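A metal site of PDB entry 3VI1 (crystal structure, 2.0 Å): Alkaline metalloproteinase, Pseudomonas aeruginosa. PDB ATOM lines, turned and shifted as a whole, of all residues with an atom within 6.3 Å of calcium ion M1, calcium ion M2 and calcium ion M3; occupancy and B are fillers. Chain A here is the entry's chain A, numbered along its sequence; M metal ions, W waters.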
ATOM      1  N   GLY A 333       1.803   7.214   1.179  1.00  0.00           N
ATOM      2  CA  GLY A 333       1.432   8.440   0.475  1.00  0.00           C
ATOM      3  C   GLY A 333      -0.078   8.638   0.434  1.00  0.00           C
ATOM      4  O   GLY A 333      -0.832   7.761   0.857  1.00  0.00           O
ATOM      5  N   GLY A 334      -0.502   9.784  -0.069  1.00  0.00           N
ATOM      6  CA  GLY A 334      -1.930  10.088  -0.199  1.00  0.00           C
ATOM      7  C   GLY A 334      -2.461   9.784  -1.590  1.00  0.00           C
ATOM      8  O   GLY A 334      -1.861   9.016  -2.335  1.00  0.00           O
ATOM      9  N   SER A 335      -3.589  10.405  -1.935  1.00  0.00           N
ATOM     10  CA  SER A 335      -4.242  10.184  -3.228  1.00  0.00           C
ATOM     11  C   SER A 335      -3.576  10.932  -4.393  1.00  0.00           C
ATOM     12  O   SER A 335      -3.874  10.665  -5.557  1.00  0.00           O
ATOM     13  CB  SER A 335      -5.731  10.519  -3.155  1.00  0.00           C
ATOM     14  OG  SER A 335      -5.933  11.862  -2.752  1.00  0.00           O
ATOM     15  N   GLY A 336      -2.672  11.861  -4.068  1.00  0.00           N
ATOM     16  CA  GLY A 336      -1.931  12.610  -5.075  1.00  0.00           C
ATOM     17  C   GLY A 336      -0.750  11.844  -5.624  1.00  0.00           C
ATOM     18  O   GLY A 336      -0.435  10.741  -5.158  1.00  0.00           O
ATOM     19  N   SER A 337      -0.095  12.421  -6.630  1.00  0.00           N
ATOM     20  CA  SER A 337       1.100  11.822  -7.213  1.00  0.00           C
ATOM     21  C   SER A 337       2.316  12.075  -6.328  1.00  0.00           C
ATOM     22  O   SER A 337       2.853  13.172  -6.291  1.00  0.00           O
ATOM     23  CB  SER A 337       1.327  12.361  -8.635  1.00  0.00           C
ATOM     24  OG  SER A 337       0.315  11.914  -9.506  1.00  0.00           O
ATOM     25  N   ASP A 338       2.729  11.032  -5.609  1.00  0.00           N
ATOM     26  CA  ASP A 338       3.723  11.174  -4.549  1.00  0.00           C
ATOM     27  C   ASP A 338       5.104  10.645  -4.912  1.00  0.00           C
ATOM     28  O   ASP A 338       5.263   9.825  -5.821  1.00  0.00           O
ATOM     29  CB  ASP A 338       3.244  10.480  -3.266  1.00  0.00           C
ATOM     30  CG  ASP A 338       1.889  10.984  -2.801  1.00  0.00           C
ATOM     31  OD1 ASP A 338       1.686  12.219  -2.758  1.00  0.00           O
ATOM     32  OD2 ASP A 338       1.028  10.133  -2.473  1.00  0.00           O
ATOM     33  N   LEU A 340       8.153   8.740  -2.901  1.00  0.00           N
ATOM     34  CA  LEU A 340       8.495   8.035  -1.670  1.00  0.00           C
ATOM     35  C   LEU A 340       9.910   7.465  -1.712  1.00  0.00           C
ATOM     36  O   LEU A 340      10.192   6.526  -2.470  1.00  0.00           O
ATOM     37  CB  LEU A 340       7.472   6.919  -1.368  1.00  0.00           C
ATOM     38  CG  LEU A 340       6.172   7.301  -0.664  1.00  0.00           C
ATOM     39  CD1 LEU A 340       5.152   7.854  -1.648  1.00  0.00           C
ATOM     40  CD2 LEU A 340       5.599   6.094   0.059  1.00  0.00           C
ATOM     41  N   LYS A 350       4.050   2.544   0.441  1.00  0.00           N
ATOM     42  CA  LYS A 350       2.738   2.485  -0.198  1.00  0.00           C
ATOM     43  C   LYS A 350       2.381   3.825  -0.834  1.00  0.00           C
ATOM     44  O   LYS A 350       2.306   4.852  -0.153  1.00  0.00           O
ATOM     45  CB  LYS A 350       1.666   2.042   0.811  1.00  0.00           C
ATOM     46  CG  LYS A 350       1.851   0.618   1.312  1.00  0.00           C
ATOM     47  CD  LYS A 350       0.688   0.150   2.162  1.00  0.00           C
ATOM     48  CE  LYS A 350       0.866  -1.309   2.546  1.00  0.00           C
ATOM     49  NZ  LYS A 350      -0.221  -1.802   3.435  1.00  0.00           N
ATOM     50  N   GLY A 351       2.182   3.807  -2.145  1.00  0.00           N
ATOM     51  CA  GLY A 351       1.903   5.021  -2.905  1.00  0.00           C
ATOM     52  C   GLY A 351       0.457   5.472  -2.841  1.00  0.00           C
ATOM     53  O   GLY A 351       0.185   6.679  -2.855  1.00  0.00           O
ATOM     54  N   GLY A 352      -0.466   4.525  -2.781  1.00  0.00           N
ATOM     55  CA  GLY A 352      -1.902   4.830  -2.813  1.00  0.00           C
ATOM     56  C   GLY A 352      -2.340   5.224  -4.211  1.00  0.00           C
ATOM     57  O   GLY A 352      -1.749   4.799  -5.198  1.00  0.00           O
ATOM     58  N   ALA A 353      -3.375   6.059  -4.287  1.00  0.00           N
ATOM     59  CA  ALA A 353      -3.869   6.569  -5.565  1.00  0.00           C
ATOM     60  C   ALA A 353      -2.873   7.551  -6.204  1.00  0.00           C
ATOM     61  O   ALA A 353      -1.963   8.040  -5.535  1.00  0.00           O
ATOM     62  CB  ALA A 353      -5.235   7.235  -5.388  1.00  0.00           C
ATOM     63  N   GLY A 354      -3.067   7.823  -7.497  1.00  0.00           N
ATOM     64  CA  GLY A 354      -2.183   8.730  -8.228  1.00  0.00           C
ATOM     65  C   GLY A 354      -0.942   8.037  -8.764  1.00  0.00           C
ATOM     66  O   GLY A 354      -0.701   6.866  -8.481  1.00  0.00           O
ATOM     67  N   ASN A 355      -0.146   8.786  -9.535  1.00  0.00           N
ATOM     68  CA  ASN A 355       1.057   8.256 -10.162  1.00  0.00           C
ATOM     69  C   ASN A 355       2.299   8.468  -9.300  1.00  0.00           C
ATOM     70  O   ASN A 355       2.888   9.552  -9.287  1.00  0.00           O
ATOM     71  CB  ASN A 355       1.243   8.870 -11.554  1.00  0.00           C
ATOM     72  CG  ASN A 355       0.096   8.557 -12.496  1.00  0.00           C
ATOM     73  OD1 ASN A 355      -0.535   7.496 -12.400  1.00  0.00           O
ATOM     74  ND2 ASN A 355      -0.180   9.470 -13.413  1.00  0.00           N
ATOM     75  N   ASP A 356       2.703   7.415  -8.599  1.00  0.00           N
ATOM     76  CA  ASP A 356       3.742   7.520  -7.585  1.00  0.00           C
ATOM     77  C   ASP A 356       5.100   6.998  -8.041  1.00  0.00           C
ATOM     78  O   ASP A 356       5.187   6.070  -8.847  1.00  0.00           O
ATOM     79  CB  ASP A 356       3.327   6.804  -6.300  1.00  0.00           C
ATOM     80  CG  ASP A 356       1.964   7.239  -5.813  1.00  0.00           C
ATOM     81  OD1 ASP A 356       1.818   8.418  -5.418  1.00  0.00           O
ATOM     82  OD2 ASP A 356       1.031   6.409  -5.810  1.00  0.00           O
ATOM     83  N   TRP A 368       4.471  -1.096  -2.636  1.00  0.00           N
ATOM     84  CA  TRP A 368       3.089  -1.074  -3.107  1.00  0.00           C
ATOM     85  C   TRP A 368       2.859   0.216  -3.890  1.00  0.00           C
ATOM     86  O   TRP A 368       3.033   1.308  -3.370  1.00  0.00           O
ATOM     87  CB  TRP A 368       2.113  -1.134  -1.921  1.00  0.00           C
ATOM     88  CG  TRP A 368       2.356  -2.280  -0.962  1.00  0.00           C
ATOM     89  CD1 TRP A 368       3.365  -2.386  -0.049  1.00  0.00           C
ATOM     90  CD2 TRP A 368       1.541  -3.451  -0.800  1.00  0.00           C
ATOM     91  NE1 TRP A 368       3.252  -3.561   0.650  1.00  0.00           N
ATOM     92  CE2 TRP A 368       2.143  -4.230   0.213  1.00  0.00           C
ATOM     93  CE3 TRP A 368       0.377  -3.927  -1.421  1.00  0.00           C
ATOM     94  CZ2 TRP A 368       1.607  -5.466   0.631  1.00  0.00           C
ATOM     95  CZ3 TRP A 368      -0.152  -5.144  -1.012  1.00  0.00           C
ATOM     96  CH2 TRP A 368       0.465  -5.893   0.010  1.00  0.00           C
ATOM     97  N   GLY A 369       2.481   0.056  -5.153  1.00  0.00           N
ATOM     98  CA  GLY A 369       2.190   1.202  -6.004  1.00  0.00           C
ATOM     99  C   GLY A 369       0.801   1.763  -5.779  1.00  0.00           C
ATOM    100  O   GLY A 369       0.599   2.981  -5.772  1.00  0.00           O
ATOM    101  N   GLY A 370      -0.168   0.874  -5.560  1.00  0.00           N
ATOM    102  CA  GLY A 370      -1.572   1.250  -5.480  1.00  0.00           C
ATOM    103  C   GLY A 370      -2.141   1.443  -6.878  1.00  0.00           C
ATOM    104  O   GLY A 370      -1.576   0.927  -7.856  1.00  0.00           O
ATOM    105  N   ALA A 371      -3.232   2.188  -6.980  1.00  0.00           N
ATOM    106  CA  ALA A 371      -3.830   2.514  -8.276  1.00  0.00           C
ATOM    107  C   ALA A 371      -2.962   3.519  -9.032  1.00  0.00           C
ATOM    108  O   ALA A 371      -2.147   4.220  -8.425  1.00  0.00           O
ATOM    109  CB  ALA A 371      -5.234   3.038  -8.100  1.00  0.00           C
ATOM    110  N   GLY A 372      -3.155   3.592 -10.341  1.00  0.00           N
ATOM    111  CA  GLY A 372      -2.410   4.529 -11.193  1.00  0.00           C
ATOM    112  C   GLY A 372      -1.088   3.966 -11.699  1.00  0.00           C
ATOM    113  O   GLY A 372      -0.675   2.874 -11.311  1.00  0.00           O
ATOM    114  N   ALA A 373      -0.438   4.730 -12.573  1.00  0.00           N
ATOM    115  CA  ALA A 373       0.844   4.343 -13.164  1.00  0.00           C
ATOM    116  C   ALA A 373       1.996   4.685 -12.236  1.00  0.00           C
ATOM    117  O   ALA A 373       2.394   5.846 -12.114  1.00  0.00           O
ATOM    118  CB  ALA A 373       1.020   5.028 -14.524  1.00  0.00           C
ATOM    119  N   ASP A 374       2.546   3.665 -11.587  1.00  0.00           N
ATOM    120  CA  ASP A 374       3.603   3.850 -10.600  1.00  0.00           C
ATOM    121  C   ASP A 374       4.966   3.412 -11.118  1.00  0.00           C
ATOM    122  O   ASP A 374       5.061   2.494 -11.928  1.00  0.00           O
ATOM    123  CB  ASP A 374       3.251   3.117  -9.303  1.00  0.00           C
ATOM    124  CG  ASP A 374       1.922   3.542  -8.732  1.00  0.00           C
ATOM    125  OD1 ASP A 374       1.803   4.688  -8.253  1.00  0.00           O
ATOM    126  OD2 ASP A 374       0.976   2.728  -8.759  1.00  0.00           O
ATOM    127  N   PHE A 376       8.857   2.197 -10.035  1.00  0.00           N
ATOM    128  CA  PHE A 376       9.755   1.656  -9.031  1.00  0.00           C
ATOM    129  C   PHE A 376      11.193   1.844  -9.512  1.00  0.00           C
ATOM    130  O   PHE A 376      11.627   1.195 -10.466  1.00  0.00           O
ATOM    131  CB  PHE A 376       9.425   0.187  -8.747  1.00  0.00           C
ATOM    132  CG  PHE A 376       7.972  -0.056  -8.418  1.00  0.00           C
ATOM    133  CD1 PHE A 376       7.082  -0.464  -9.413  1.00  0.00           C
ATOM    134  CD2 PHE A 376       7.493   0.155  -7.124  1.00  0.00           C
ATOM    135  CE1 PHE A 376       5.736  -0.680  -9.114  1.00  0.00           C
ATOM    136  CE2 PHE A 376       6.146  -0.061  -6.825  1.00  0.00           C
ATOM    137  CZ  PHE A 376       5.268  -0.477  -7.815  1.00  0.00           C
ATOM    138  N   ASP A 394       2.064  -5.250  -5.816  1.00  0.00           N
ATOM    139  CA  ASP A 394       0.849  -5.043  -6.610  1.00  0.00           C
ATOM    140  C   ASP A 394       1.136  -4.562  -8.034  1.00  0.00           C
ATOM    141  O   ASP A 394       0.431  -3.699  -8.560  1.00  0.00           O
ATOM    142  CB  ASP A 394      -0.133  -4.100  -5.880  1.00  0.00           C
ATOM    143  CG  ASP A 394       0.478  -2.727  -5.583  1.00  0.00           C
ATOM    144  OD1 ASP A 394       1.633  -2.463  -5.970  1.00  0.00           O
ATOM    145  OD2 ASP A 394      -0.225  -1.902  -4.959  1.00  0.00           O
ATOM    146  N   VAL A 396       1.178  -4.097 -11.859  1.00  0.00           N
ATOM    147  CA  VAL A 396       0.249  -4.274 -12.965  1.00  0.00           C
ATOM    148  C   VAL A 396       0.986  -4.000 -14.278  1.00  0.00           C
ATOM    149  O   VAL A 396       1.508  -2.905 -14.496  1.00  0.00           O
ATOM    150  CB  VAL A 396      -0.981  -3.323 -12.851  1.00  0.00           C
ATOM    151  CG1 VAL A 396      -1.945  -3.545 -14.016  1.00  0.00           C
ATOM    152  CG2 VAL A 396      -1.698  -3.526 -11.516  1.00  0.00           C
ATOM    153  N   GLN A 399       0.925  -0.714 -16.981  1.00  0.00           N
ATOM    154  CA  GLN A 399       0.575   0.463 -16.196  1.00  0.00           C
ATOM    155  C   GLN A 399       1.752   0.896 -15.321  1.00  0.00           C
ATOM    156  O   GLN A 399       2.186   2.056 -15.375  1.00  0.00           O
ATOM    157  CB  GLN A 399      -0.660   0.201 -15.337  1.00  0.00           C
ATOM    158  CG  GLN A 399      -1.266   1.444 -14.697  1.00  0.00           C
ATOM    159  CD  GLN A 399      -2.421   1.134 -13.755  1.00  0.00           C
ATOM    160  OE1 GLN A 399      -2.391   0.144 -13.026  1.00  0.00           O
ATOM    161  NE2 GLN A 399      -3.427   1.995 -13.764  1.00  0.00           N
ATOM    162  N   ASP A 400       2.271  -0.037 -14.527  1.00  0.00           N
ATOM    163  CA  ASP A 400       3.424   0.225 -13.671  1.00  0.00           C
ATOM    164  C   ASP A 400       4.725   0.084 -14.434  1.00  0.00           C
ATOM    165  O   ASP A 400       4.766  -0.526 -15.517  1.00  0.00           O
ATOM    166  CB  ASP A 400       3.418  -0.720 -12.466  1.00  0.00           C
ATOM    167  CG  ASP A 400       2.222  -0.516 -11.561  1.00  0.00           C
ATOM    168  OD1 ASP A 400       1.790   0.650 -11.374  1.00  0.00           O
ATOM    169  OD2 ASP A 400       1.713  -1.519 -11.020  1.00  0.00           O
HETATM  170 CA    CA M   1      -0.317   4.883  -7.071  1.00  0.00          CA
HETATM  171 CA    CA M   2      -0.212   8.647  -4.036  1.00  0.00          CA
HETATM  172 CA    CA M   3      -0.183   0.997  -9.791  1.00  0.00          CA
HETATM  173  O   HOH W   1       1.078  -0.723  -8.538  1.00  0.00           O
HETATM  174  O   HOH W   2      -2.126  -0.312 -10.354  1.00  0.00           O
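Calcium ion M2 is bound by the backbone carbonyl oxygen (O) of Gly 351 (2.3 Å), the backbone carbonyl oxygen (O) of Ala 353 (2.4 Å), the backbone carbonyl oxygen (O) of Gly 336 (2.4 Å), the backbone carbonyl oxygen (O) of Gly 334 (2.4 Å), the side-chain carboxylate (OD1) of Asp 356 (2.5 Å) and the side-chain carboxylate (OD2) of Asp 338 (2.5 Å). Calcium ion M2 has six donor atoms within binding distance. Slightly farther from calcium ion M2 lies OD2 of Asp 356 (3.1 Å).
Of the 26 residues printed, 8 come within 4 Å of calcium ion M1.
The nearest printed residue that does not touch calcium ion M2 is Gly 352 (4.03 Å).
The side-chain carboxylate (OD1) of Asp 394 lies within hydrogen-bond range of the backbone NH (N) of Gly 369, at 2.8 Å. N of Val 396 lies within hydrogen-bond range of OD2 of Asp 400 (2.8 Å). The backbone NH of Gly 351 is in hydrogen-bond range of the backbone carbonyl oxygen of Trp 368 (2.9 Å). N of Gly 370 lies within hydrogen-bond range of OD2 of Asp 394, at 2.8 Å.
Water W1 bridges OD2 of Asp 400 (2.7 Å) and O of Asp 394 (3.0 Å).
Calcium ion M3 is bound by OD2 of Asp 374, 2.3 Å away. Calcium ion M3 is bound by O of Gly 370, 2.4 Å away. Water W2 is bound to calcium ion M3 (2.4 Å). The backbone carbonyl oxygen (O) of Gly 372 is bound to calcium ion M3, at 2.5 Å. Water W1 binds calcium ion M3. The side-chain carboxylate (OD1) of Asp 400 is bound to calcium ion M3, 2.6 Å away. Calcium ion M3 has six donor atoms within binding distance.
Calcium ion M1 is bound by the backbone carbonyl oxygen (O) of Gly 352 (2.4 Å). Calcium ion M1 is bound by O of Ala 371 (2.4 Å). OD2 of Asp 356 is bound to calcium ion M1, at 2.4 Å. OD1 of Asp 374 is bound to calcium ion M1 (2.4 Å). O of Gly 354 binds calcium ion M1 (2.5 Å). O of Gly 369 binds calcium ion M1 (2.5 Å). Calcium ion M1 has six donor atoms within binding distance. Slightly farther from calcium ion M1 lies the side-chain carboxylate (OD2) of Asp 374 (3.0 Å).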
